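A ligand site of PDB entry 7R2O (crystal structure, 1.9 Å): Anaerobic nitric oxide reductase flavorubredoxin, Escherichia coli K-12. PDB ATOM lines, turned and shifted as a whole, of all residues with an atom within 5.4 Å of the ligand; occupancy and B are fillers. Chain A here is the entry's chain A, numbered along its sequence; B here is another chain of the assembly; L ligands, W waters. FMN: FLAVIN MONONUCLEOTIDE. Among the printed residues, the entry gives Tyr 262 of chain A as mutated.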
ATOM      1  N   ASP A 259      11.550  38.992 -12.927  1.00  0.00           N
ATOM      2  CA  ASP A 259      10.669  38.923 -14.078  1.00  0.00           C
ATOM      3  C   ASP A 259       9.983  37.568 -14.048  1.00  0.00           C
ATOM      4  O   ASP A 259      10.511  36.608 -13.492  1.00  0.00           O
ATOM      5  CB  ASP A 259      11.418  39.133 -15.401  1.00  0.00           C
ATOM      6  CG  ASP A 259      10.535  39.694 -16.504  1.00  0.00           C
ATOM      7  OD1 ASP A 259       9.289  39.693 -16.334  1.00  0.00           O
ATOM      8  OD2 ASP A 259      11.080  40.155 -17.522  1.00  0.00           O
ATOM      9  N   THR A 260       8.791  37.503 -14.638  1.00  0.00           N
ATOM     10  CA  THR A 260       7.973  36.307 -14.526  1.00  0.00           C
ATOM     11  C   THR A 260       7.096  36.195 -15.768  1.00  0.00           C
ATOM     12  O   THR A 260       6.701  37.211 -16.356  1.00  0.00           O
ATOM     13  CB  THR A 260       7.112  36.341 -13.265  1.00  0.00           C
ATOM     14  OG1 THR A 260       6.421  35.089 -13.117  1.00  0.00           O
ATOM     15  CG2 THR A 260       6.086  37.456 -13.345  1.00  0.00           C
ATOM     16  N   MET A 261       6.812  34.957 -16.157  1.00  0.00           N
ATOM     17  CA  MET A 261       5.951  34.688 -17.302  1.00  0.00           C
ATOM     18  C   MET A 261       4.552  34.257 -16.915  1.00  0.00           C
ATOM     19  O   MET A 261       3.598  34.539 -17.647  1.00  0.00           O
ATOM     20  CB  MET A 261       6.580  33.626 -18.209  1.00  0.00           C
ATOM     21  CG  MET A 261       7.861  34.062 -18.877  1.00  0.00           C
ATOM     22  SD  MET A 261       8.547  32.825 -19.974  1.00  0.00           S
ATOM     23  CE  MET A 261       8.970  31.523 -18.812  1.00  0.00           C
ATOM     24  N   TYR A 262       4.393  33.568 -15.784  1.00  0.00           N
ATOM     25  CA  TYR A 262       3.093  33.082 -15.348  1.00  0.00           C
ATOM     26  C   TYR A 262       2.841  33.366 -13.866  1.00  0.00           C
ATOM     27  O   TYR A 262       1.953  32.756 -13.272  1.00  0.00           O
ATOM     28  CB  TYR A 262       2.947  31.593 -15.652  1.00  0.00           C
ATOM     29  CG  TYR A 262       2.787  31.324 -17.136  1.00  0.00           C
ATOM     30  CD1 TYR A 262       1.644  31.724 -17.815  1.00  0.00           C
ATOM     31  CD2 TYR A 262       3.780  30.677 -17.865  1.00  0.00           C
ATOM     32  CE1 TYR A 262       1.480  31.496 -19.163  1.00  0.00           C
ATOM     33  CE2 TYR A 262       3.630  30.429 -19.227  1.00  0.00           C
ATOM     34  CZ  TYR A 262       2.477  30.845 -19.868  1.00  0.00           C
ATOM     35  OH  TYR A 262       2.314  30.617 -21.215  1.00  0.00           O
ATOM     36  N   ASN A 263       3.606  34.289 -13.279  1.00  0.00           N
ATOM     37  CA  ASN A 263       3.439  34.807 -11.934  1.00  0.00           C
ATOM     38  C   ASN A 263       3.952  33.854 -10.853  1.00  0.00           C
ATOM     39  O   ASN A 263       3.829  34.173  -9.662  1.00  0.00           O
ATOM     40  CB  ASN A 263       1.975  35.165 -11.613  1.00  0.00           C
ATOM     41  CG  ASN A 263       1.549  36.445 -12.282  1.00  0.00           C
ATOM     42  OD1 ASN A 263       2.315  37.403 -12.361  1.00  0.00           O
ATOM     43  ND2 ASN A 263       0.307  36.465 -12.774  1.00  0.00           N
ATOM     44  N   ASN A 264       4.526  32.712 -11.221  1.00  0.00           N
ATOM     45  CA  ASN A 264       5.025  31.788 -10.209  1.00  0.00           C
ATOM     46  C   ASN A 264       6.179  32.406  -9.439  1.00  0.00           C
ATOM     47  O   ASN A 264       6.166  32.418  -8.199  1.00  0.00           O
ATOM     48  CB  ASN A 264       5.422  30.474 -10.876  1.00  0.00           C
ATOM     49  CG  ASN A 264       4.245  29.774 -11.526  1.00  0.00           C
ATOM     50  OD1 ASN A 264       3.177  29.666 -10.944  1.00  0.00           O
ATOM     51  ND2 ASN A 264       4.439  29.315 -12.757  1.00  0.00           N
ATOM     52  N   THR A 265       7.179  32.925 -10.147  1.00  0.00           N
ATOM     53  CA  THR A 265       8.272  33.634  -9.481  1.00  0.00           C
ATOM     54  C   THR A 265       7.749  34.828  -8.685  1.00  0.00           C
ATOM     55  O   THR A 265       8.306  35.165  -7.639  1.00  0.00           O
ATOM     56  CB  THR A 265       9.313  34.071 -10.513  1.00  0.00           C
ATOM     57  OG1 THR A 265       9.844  32.926 -11.189  1.00  0.00           O
ATOM     58  CG2 THR A 265      10.463  34.810  -9.835  1.00  0.00           C
ATOM     59  N   ARG A 266       6.675  35.462  -9.162  1.00  0.00           N
ATOM     60  CA  ARG A 266       6.053  36.554  -8.416  1.00  0.00           C
ATOM     61  C   ARG A 266       5.489  36.057  -7.097  1.00  0.00           C
ATOM     62  O   ARG A 266       5.641  36.719  -6.051  1.00  0.00           O
ATOM     63  CB  ARG A 266       4.972  37.217  -9.265  1.00  0.00           C
ATOM     64  CG  ARG A 266       4.308  38.428  -8.617  1.00  0.00           C
ATOM     65  CD  ARG A 266       2.876  38.133  -8.214  1.00  0.00           C
ATOM     66  NE  ARG A 266       2.233  39.323  -7.671  1.00  0.00           N
ATOM     67  CZ  ARG A 266       1.635  40.246  -8.413  1.00  0.00           C
ATOM     68  NH1 ARG A 266       1.082  41.312  -7.830  1.00  0.00           N
ATOM     69  NH2 ARG A 266       1.582  40.114  -9.731  1.00  0.00           N
ATOM     70  N   SER A 313      12.369  33.135 -13.751  1.00  0.00           N
ATOM     71  CA  SER A 313      12.032  31.801 -14.209  1.00  0.00           C
ATOM     72  C   SER A 313      13.061  31.369 -15.250  1.00  0.00           C
ATOM     73  O   SER A 313      13.808  32.184 -15.794  1.00  0.00           O
ATOM     74  CB  SER A 313      10.612  31.757 -14.772  1.00  0.00           C
ATOM     75  OG  SER A 313      10.322  32.909 -15.562  1.00  0.00           O
ATOM     76  N   THR A 314      13.107  30.061 -15.508  1.00  0.00           N
ATOM     77  CA  THR A 314      13.990  29.534 -16.529  1.00  0.00           C
ATOM     78  C   THR A 314      13.274  29.531 -17.867  1.00  0.00           C
ATOM     79  O   THR A 314      12.166  28.993 -17.999  1.00  0.00           O
ATOM     80  CB  THR A 314      14.491  28.132 -16.179  1.00  0.00           C
ATOM     81  OG1 THR A 314      15.292  28.190 -14.990  1.00  0.00           O
ATOM     82  CG2 THR A 314      15.330  27.558 -17.318  1.00  0.00           C
ATOM     83  N   MET A 315      13.909  30.146 -18.860  1.00  0.00           N
ATOM     84  CA  MET A 315      13.384  30.213 -20.221  1.00  0.00           C
ATOM     85  C   MET A 315      14.515  29.804 -21.150  1.00  0.00           C
ATOM     86  O   MET A 315      15.491  30.538 -21.311  1.00  0.00           O
ATOM     87  CB  MET A 315      12.875  31.619 -20.527  1.00  0.00           C
ATOM     88  CG  MET A 315      12.988  32.035 -21.967  1.00  0.00           C
ATOM     89  SD  MET A 315      12.146  33.598 -22.289  1.00  0.00           S
ATOM     90  CE  MET A 315      10.491  32.983 -22.599  1.00  0.00           C
ATOM     91  N   ASN A 316      14.407  28.599 -21.721  1.00  0.00           N
ATOM     92  CA  ASN A 316      15.437  28.069 -22.635  1.00  0.00           C
ATOM     93  C   ASN A 316      16.784  27.892 -21.944  1.00  0.00           C
ATOM     94  O   ASN A 316      17.829  28.141 -22.536  1.00  0.00           O
ATOM     95  CB  ASN A 316      15.611  28.959 -23.866  1.00  0.00           C
ATOM     96  CG  ASN A 316      14.366  29.064 -24.679  1.00  0.00           C
ATOM     97  OD1 ASN A 316      13.675  28.081 -24.899  1.00  0.00           O
ATOM     98  ND2 ASN A 316      14.070  30.267 -25.124  1.00  0.00           N
ATOM     99  N   ASN A 317      16.764  27.456 -20.696  1.00  0.00           N
ATOM    100  CA  ASN A 317      17.886  27.182 -19.808  1.00  0.00           C
ATOM    101  C   ASN A 317      18.585  28.455 -19.328  1.00  0.00           C
ATOM    102  O   ASN A 317      19.434  28.350 -18.469  1.00  0.00           O
ATOM    103  CB  ASN A 317      18.938  26.245 -20.435  1.00  0.00           C
ATOM    104  CG  ASN A 317      18.349  24.930 -20.929  1.00  0.00           C
ATOM    105  OD1 ASN A 317      17.443  24.370 -20.323  1.00  0.00           O
ATOM    106  ND2 ASN A 317      18.825  24.462 -22.111  1.00  0.00           N
ATOM    107  N   SER A 345      11.118  30.193 -10.320  1.00  0.00           N
ATOM    108  CA  SER A 345      10.385  28.988 -10.661  1.00  0.00           C
ATOM    109  C   SER A 345      10.877  28.407 -11.990  1.00  0.00           C
ATOM    110  O   SER A 345      11.317  29.131 -12.880  1.00  0.00           O
ATOM    111  CB  SER A 345       8.889  29.291 -10.746  1.00  0.00           C
ATOM    112  OG  SER A 345       8.171  28.209 -11.317  1.00  0.00           O
ATOM    113  N   HIS A 346      10.782  27.082 -12.112  1.00  0.00           N
ATOM    114  CA  HIS A 346      11.213  26.386 -13.311  1.00  0.00           C
ATOM    115  C   HIS A 346      10.236  25.256 -13.604  1.00  0.00           C
ATOM    116  O   HIS A 346       9.502  24.797 -12.732  1.00  0.00           O
ATOM    117  CB  HIS A 346      12.630  25.815 -13.163  1.00  0.00           C
ATOM    118  CG  HIS A 346      12.731  24.741 -12.120  1.00  0.00           C
ATOM    119  ND1 HIS A 346      13.177  24.994 -10.840  1.00  0.00           N
ATOM    120  CD2 HIS A 346      12.417  23.430 -12.167  1.00  0.00           C
ATOM    121  CE1 HIS A 346      13.147  23.872 -10.139  1.00  0.00           C
ATOM    122  NE2 HIS A 346      12.685  22.909 -10.922  1.00  0.00           N
ATOM    123  N   GLY A 347      10.245  24.807 -14.863  1.00  0.00           N
ATOM    124  CA  GLY A 347       9.355  23.740 -15.288  1.00  0.00           C
ATOM    125  C   GLY A 347       9.923  22.347 -15.095  1.00  0.00           C
ATOM    126  O   GLY A 347       9.199  21.434 -14.685  1.00  0.00           O
ATOM    127  N   TRP A 348      11.212  22.159 -15.378  1.00  0.00           N
ATOM    128  CA  TRP A 348      11.791  20.831 -15.252  1.00  0.00           C
ATOM    129  C   TRP A 348      13.220  20.859 -14.728  1.00  0.00           C
ATOM    130  O   TRP A 348      13.447  20.592 -13.547  1.00  0.00           O
ATOM    131  CB  TRP A 348      11.727  20.092 -16.596  1.00  0.00           C
ATOM    132  CG  TRP A 348      12.101  20.906 -17.791  1.00  0.00           C
ATOM    133  CD1 TRP A 348      13.305  20.927 -18.424  1.00  0.00           C
ATOM    134  CD2 TRP A 348      11.251  21.808 -18.538  1.00  0.00           C
ATOM    135  NE1 TRP A 348      13.269  21.781 -19.501  1.00  0.00           N
ATOM    136  CE2 TRP A 348      12.022  22.331 -19.591  1.00  0.00           C
ATOM    137  CE3 TRP A 348       9.919  22.206 -18.398  1.00  0.00           C
ATOM    138  CZ2 TRP A 348      11.504  23.242 -20.505  1.00  0.00           C
ATOM    139  CZ3 TRP A 348       9.411  23.116 -19.301  1.00  0.00           C
ATOM    140  CH2 TRP A 348      10.197  23.627 -20.351  1.00  0.00           C
ATOM    141  N   SER A 349      14.194  21.167 -15.588  1.00  0.00           N
ATOM    142  CA  SER A 349      15.590  21.087 -15.196  1.00  0.00           C
ATOM    143  C   SER A 349      16.149  22.382 -14.633  1.00  0.00           C
ATOM    144  O   SER A 349      17.305  22.397 -14.204  1.00  0.00           O
ATOM    145  CB  SER A 349      16.438  20.629 -16.393  1.00  0.00           C
ATOM    146  OG  SER A 349      16.181  21.433 -17.532  1.00  0.00           O
ATOM    147  N   GLY A 350      15.373  23.461 -14.613  1.00  0.00           N
ATOM    148  CA  GLY A 350      15.855  24.706 -14.027  1.00  0.00           C
ATOM    149  C   GLY A 350      17.195  25.136 -14.597  1.00  0.00           C
ATOM    150  O   GLY A 350      17.471  24.945 -15.791  1.00  0.00           O
ATOM    151  N   LYS A 374       9.281  24.446  -8.276  1.00  0.00           N
ATOM    152  CA  LYS A 374       8.801  23.873  -9.517  1.00  0.00           C
ATOM    153  C   LYS A 374       7.378  24.360  -9.791  1.00  0.00           C
ATOM    154  O   LYS A 374       6.527  24.325  -8.901  1.00  0.00           O
ATOM    155  CB  LYS A 374       8.861  22.347  -9.469  1.00  0.00           C
ATOM    156  CG  LYS A 374       8.868  21.668 -10.828  1.00  0.00           C
ATOM    157  CD  LYS A 374       9.005  20.157 -10.694  1.00  0.00           C
ATOM    158  CE  LYS A 374       9.059  19.489 -12.064  1.00  0.00           C
ATOM    159  NZ  LYS A 374       9.277  18.021 -11.984  1.00  0.00           N
ATOM    160  N   TRP A 375       7.139  24.823 -11.022  1.00  0.00           N
ATOM    161  CA  TRP A 375       5.821  25.303 -11.450  1.00  0.00           C
ATOM    162  C   TRP A 375       5.220  26.294 -10.455  1.00  0.00           C
ATOM    163  O   TRP A 375       5.935  27.133  -9.910  1.00  0.00           O
ATOM    164  CB  TRP A 375       4.875  24.116 -11.675  1.00  0.00           C
ATOM    165  CG  TRP A 375       5.369  23.096 -12.676  1.00  0.00           C
ATOM    166  CD1 TRP A 375       5.599  21.767 -12.442  1.00  0.00           C
ATOM    167  CD2 TRP A 375       5.689  23.312 -14.064  1.00  0.00           C
ATOM    168  NE1 TRP A 375       6.032  21.143 -13.587  1.00  0.00           N
ATOM    169  CE2 TRP A 375       6.102  22.064 -14.597  1.00  0.00           C
ATOM    170  CE3 TRP A 375       5.669  24.426 -14.901  1.00  0.00           C
ATOM    171  CZ2 TRP A 375       6.496  21.910 -15.923  1.00  0.00           C
ATOM    172  CZ3 TRP A 375       6.063  24.272 -16.227  1.00  0.00           C
ATOM    173  CH2 TRP A 375       6.467  23.023 -16.725  1.00  0.00           C
ATOM    174  N   ARG A 376       3.908  26.205 -10.213  1.00  0.00           N
ATOM    175  CA  ARG A 376       3.253  27.132  -9.281  1.00  0.00           C
ATOM    176  C   ARG A 376       3.399  26.618  -7.857  1.00  0.00           C
ATOM    177  O   ARG A 376       2.986  25.489  -7.567  1.00  0.00           O
ATOM    178  CB  ARG A 376       1.778  27.315  -9.612  1.00  0.00           C
ATOM    179  CG  ARG A 376       1.059  28.213  -8.602  1.00  0.00           C
ATOM    180  CD  ARG A 376      -0.304  28.678  -9.097  1.00  0.00           C
ATOM    181  NE  ARG A 376      -1.315  27.618  -9.028  1.00  0.00           N
ATOM    182  CZ  ARG A 376      -2.084  27.378  -7.979  1.00  0.00           C
ATOM    183  NH1 ARG A 376      -1.974  28.121  -6.879  1.00  0.00           N
ATOM    184  NH2 ARG A 376      -2.973  26.389  -8.005  1.00  0.00           N
ATOM    185  N   HIS B  23       4.605  35.244 -22.763  1.00  0.00           N
ATOM    186  CA  HIS B  23       5.847  34.905 -22.058  1.00  0.00           C
ATOM    187  C   HIS B  23       6.298  36.079 -21.176  1.00  0.00           C
ATOM    188  O   HIS B  23       7.446  36.514 -21.210  1.00  0.00           O
ATOM    189  CB  HIS B  23       6.952  34.528 -23.044  1.00  0.00           C
ATOM    190  CG  HIS B  23       6.626  33.331 -23.885  1.00  0.00           C
ATOM    191  ND1 HIS B  23       5.594  32.462 -23.572  1.00  0.00           N
ATOM    192  CD2 HIS B  23       7.197  32.856 -25.019  1.00  0.00           C
ATOM    193  CE1 HIS B  23       5.550  31.502 -24.485  1.00  0.00           C
ATOM    194  NE2 HIS B  23       6.505  31.721 -25.377  1.00  0.00           N
ATOM    195  N   GLU B  81       0.621  24.037 -20.571  1.00  0.00           N
ATOM    196  CA  GLU B  81       0.886  25.454 -20.414  1.00  0.00           C
ATOM    197  C   GLU B  81      -0.435  26.196 -20.187  1.00  0.00           C
ATOM    198  O   GLU B  81      -1.479  25.813 -20.716  1.00  0.00           O
ATOM    199  CB  GLU B  81       1.625  26.021 -21.631  1.00  0.00           C
ATOM    200  CG  GLU B  81       2.241  27.406 -21.421  1.00  0.00           C
ATOM    201  CD  GLU B  81       3.314  27.728 -22.456  1.00  0.00           C
ATOM    202  OE1 GLU B  81       3.805  26.796 -23.120  1.00  0.00           O
ATOM    203  OE2 GLU B  81       3.665  28.922 -22.603  1.00  0.00           O
ATOM    204  N   HIS B 113       0.607  23.126 -11.942  1.00  0.00           N
ATOM    205  CA  HIS B 113      -0.179  24.351 -12.026  1.00  0.00           C
ATOM    206  C   HIS B 113      -1.474  24.290 -11.228  1.00  0.00           C
ATOM    207  O   HIS B 113      -1.836  25.252 -10.549  1.00  0.00           O
ATOM    208  CB  HIS B 113      -0.507  24.683 -13.484  1.00  0.00           C
ATOM    209  CG  HIS B 113       0.680  25.055 -14.322  1.00  0.00           C
ATOM    210  ND1 HIS B 113       1.435  24.124 -14.995  1.00  0.00           N
ATOM    211  CD2 HIS B 113       1.224  26.267 -14.601  1.00  0.00           C
ATOM    212  CE1 HIS B 113       2.406  24.743 -15.649  1.00  0.00           C
ATOM    213  NE2 HIS B 113       2.297  26.037 -15.432  1.00  0.00           N
ATOM    214  N   HIS B 147       6.958  22.012 -27.424  1.00  0.00           N
ATOM    215  CA  HIS B 147       8.202  22.600 -26.917  1.00  0.00           C
ATOM    216  C   HIS B 147       8.426  22.340 -25.437  1.00  0.00           C
ATOM    217  O   HIS B 147       9.409  22.823 -24.872  1.00  0.00           O
ATOM    218  CB  HIS B 147       8.195  24.118 -27.170  1.00  0.00           C
ATOM    219  CG  HIS B 147       7.147  24.845 -26.385  1.00  0.00           C
ATOM    220  ND1 HIS B 147       7.444  25.638 -25.297  1.00  0.00           N
ATOM    221  CD2 HIS B 147       5.796  24.879 -26.523  1.00  0.00           C
ATOM    222  CE1 HIS B 147       6.323  26.149 -24.811  1.00  0.00           C
ATOM    223  NE2 HIS B 147       5.313  25.701 -25.526  1.00  0.00           N
ATOM    224  N   TRP B 148       7.519  21.607 -24.814  1.00  0.00           N
ATOM    225  CA  TRP B 148       7.632  21.273 -23.397  1.00  0.00           C
ATOM    226  C   TRP B 148       7.815  19.777 -23.198  1.00  0.00           C
ATOM    227  O   TRP B 148       7.515  18.972 -24.089  1.00  0.00           O
ATOM    228  CB  TRP B 148       6.387  21.723 -22.609  1.00  0.00           C
ATOM    229  CG  TRP B 148       6.493  23.121 -22.031  1.00  0.00           C
ATOM    230  CD1 TRP B 148       7.405  24.079 -22.363  1.00  0.00           C
ATOM    231  CD2 TRP B 148       5.654  23.688 -21.024  1.00  0.00           C
ATOM    232  NE1 TRP B 148       7.180  25.217 -21.630  1.00  0.00           N
ATOM    233  CE2 TRP B 148       6.106  25.006 -20.795  1.00  0.00           C
ATOM    234  CE3 TRP B 148       4.551  23.224 -20.296  1.00  0.00           C
ATOM    235  CZ2 TRP B 148       5.499  25.856 -19.876  1.00  0.00           C
ATOM    236  CZ3 TRP B 148       3.953  24.069 -19.375  1.00  0.00           C
ATOM    237  CH2 TRP B 148       4.437  25.370 -19.176  1.00  0.00           C
ATOM    238  N   ILE B 198      10.325  30.847 -30.628  1.00  0.00           N
ATOM    239  CA  ILE B 198       9.923  29.800 -29.696  1.00  0.00           C
ATOM    240  C   ILE B 198      10.628  28.482 -29.982  1.00  0.00           C
ATOM    241  O   ILE B 198      11.128  27.828 -29.070  1.00  0.00           O
ATOM    242  CB  ILE B 198       8.388  29.598 -29.697  1.00  0.00           C
ATOM    243  CG1 ILE B 198       7.663  30.940 -29.521  1.00  0.00           C
ATOM    244  CG2 ILE B 198       7.985  28.622 -28.598  1.00  0.00           C
ATOM    245  CD1 ILE B 198       7.958  31.608 -28.214  1.00  0.00           C
HETATM  246  N1  FMN L   1      11.617  25.330 -17.511  1.00  0.00           N
HETATM  247  C2  FMN L   1      12.853  24.737 -17.343  1.00  0.00           C
HETATM  248  O2  FMN L   1      13.088  24.094 -16.326  1.00  0.00           O
HETATM  249  N3  FMN L   1      13.832  24.877 -18.311  1.00  0.00           N
HETATM  250  C4  FMN L   1      13.574  25.606 -19.457  1.00  0.00           C
HETATM  251  O4  FMN L   1      14.445  25.718 -20.309  1.00  0.00           O
HETATM  252  C4A FMN L   1      12.329  26.200 -19.636  1.00  0.00           C
HETATM  253  N5  FMN L   1      12.066  26.922 -20.778  1.00  0.00           N
HETATM  254  C5A FMN L   1      10.830  27.515 -20.947  1.00  0.00           C
HETATM  255  C6  FMN L   1      10.558  28.242 -22.091  1.00  0.00           C
HETATM  256  C7  FMN L   1       9.313  28.836 -22.271  1.00  0.00           C
HETATM  257  C7M FMN L   1       9.020  29.626 -23.510  1.00  0.00           C
HETATM  258  C8  FMN L   1       8.330  28.698 -21.281  1.00  0.00           C
HETATM  259  C8M FMN L   1       6.993  29.335 -21.470  1.00  0.00           C
HETATM  260  C9  FMN L   1       8.604  27.958 -20.131  1.00  0.00           C
HETATM  261  C9A FMN L   1       9.846  27.372 -19.966  1.00  0.00           C
HETATM  262  N10 FMN L   1      10.125  26.639 -18.820  1.00  0.00           N
HETATM  263  C10 FMN L   1      11.359  26.059 -18.657  1.00  0.00           C
HETATM  264  C1' FMN L   1       9.094  26.456 -17.758  1.00  0.00           C
HETATM  265  C2' FMN L   1       9.012  27.678 -16.847  1.00  0.00           C
HETATM  266  O2' FMN L   1      10.240  27.872 -16.180  1.00  0.00           O
HETATM  267  C3' FMN L   1       7.890  27.413 -15.857  1.00  0.00           C
HETATM  268  O3' FMN L   1       6.656  27.560 -16.535  1.00  0.00           O
HETATM  269  C4' FMN L   1       7.934  28.345 -14.651  1.00  0.00           C
HETATM  270  O4' FMN L   1       7.108  27.819 -13.634  1.00  0.00           O
HETATM  271  C5' FMN L   1       7.439  29.732 -15.018  1.00  0.00           C
HETATM  272  O5' FMN L   1       7.783  30.627 -13.985  1.00  0.00           O
HETATM  273  P   FMN L   1       7.139  32.092 -13.946  1.00  0.00           P
HETATM  274  O1P FMN L   1       7.652  32.784 -12.700  1.00  0.00           O
HETATM  275  O2P FMN L   1       7.561  32.836 -15.191  1.00  0.00           O
HETATM  276  O3P FMN L   1       5.626  32.019 -13.867  1.00  0.00           O
HETATM  277  O   HOH W   1      10.222  25.283 -23.577  1.00  0.00           O
HETATM  278  O   HOH W   2       4.392  27.912 -15.345  1.00  0.00           O
HETATM  279  O   HOH W   3      13.175  25.582 -23.388  1.00  0.00           O
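N of Met 261 lies within hydrogen-bond range of O2P of the ligand (2.4 Å). O4' of the ligand lies within hydrogen-bond range of OG of Ser 345 (2.6 Å). An oxygen (O1P) of the ligand lies within hydrogen-bond range of the backbone NH (N) of Thr 265. The side-chain hydroxyl (OG1) of Thr 265 is in hydrogen-bond range of an oxygen (O1P) of the ligand (2.7 Å). An oxygen (O1P) of the ligand lies within hydrogen-bond range of the side-chain hydroxyl (OG1) of Thr 260, 2.6 Å away. N of Tyr 262 is in hydrogen-bond range of O3P of the ligand. The side-chain hydroxyl (OG) of Ser 313 lies within hydrogen-bond range of an oxygen (O2P) of the ligand (2.8 Å). An oxygen (O2) of the ligand sits at hydrogen-bond distance from the backbone NH (N) of Trp 348, at 2.9 Å. The backbone carbonyl oxygen (O) of Thr 314 is in hydrogen-bond range of an oxygen (O2') of the ligand (2.9 Å). O4 of the ligand lies within hydrogen-bond range of N of Asn 317, 2.9 Å away. The side-chain amide oxygen of Asn 317 sits close to an oxygen (O4) of the ligand (3.3 Å). N of Gly 350 lies within hydrogen-bond range of O2 of the ligand (2.9 Å). The backbone NH (N) of Asn 264 sits at hydrogen-bond distance from an oxygen (O3P) of the ligand (2.9 Å). An oxygen (O3P) of the ligand sits at hydrogen-bond distance from the side-chain amide nitrogen of Asn 264, 3.2 Å away. N of Gly 347 lies within hydrogen-bond range of N1 of the ligand, 3.0 Å away. A nitrogen (N5) of the ligand lies within hydrogen-bond range of the backbone NH (N) of Asn 316 (3.0 Å). O3P of the ligand is in hydrogen-bond range of N of Asn 263 (3.1 Å). The backbone NH of Ser 349 is in hydrogen-bond range of an oxygen (O2) of the ligand.
The backbone NH of Ser 345 sits at hydrogen-bond distance from the side-chain hydroxyl of Thr 265. The backbone NH (N) of Thr 314 sits at hydrogen-bond distance from the backbone carbonyl oxygen (O) of Ser 345 (3.3 Å). OG of Ser 345 is in hydrogen-bond range of O of Trp 375. The side-chain hydroxyl (OG1) of Thr 260 lies within hydrogen-bond range of the backbone NH (N) of Asn 263, at 2.9 Å. OH of Tyr 262 lies within hydrogen-bond range of OE2 of Glu 81 of chain B (2.6 Å). The backbone carbonyl oxygen (O) of Gly 347 lies close to the indole nitrogen (NE1) of Trp 375. O of His 346 lies within hydrogen-bond range of N of Trp 375, 2.9 Å away.
Met 315 touches the ligand. His 346 touches the ligand. Trp 375 touches the ligand (CZ3 to O3', 3.4 Å). His 23 of chain B touches the ligand (NE2 to C7M, 3.8 Å). OE2 of Glu 81 of chain B touches C8M of the ligand (3.5 Å). NE1 of Trp 148 of chain B touches C9 of the ligand, 3.4 Å away. Within 4 Å of the ligand: Thr 260, Met 261, Tyr 262, Asn 263, Asn 264, Thr 265, Ser 313, Thr 314, Met 315, Asn 316, Asn 317, Ser 345, His 346, Gly 347, Trp 348, Ser 349, Gly 350, Trp 375, His 23 of chain B, Glu 81 of chain B and Trp 148 of chain B. The nearest printed residue that does not touch the ligand is Arg 266 (4.5 Å).
Water W2 lies within hydrogen-bond range of O3' of the ligand, NE2 of His 113 of chain B and ND2 of Asn 264. Water W3 lies within hydrogen-bond range of OD1 of Asn 316 (3.0 Å) and N5 of the ligand (3.1 Å).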
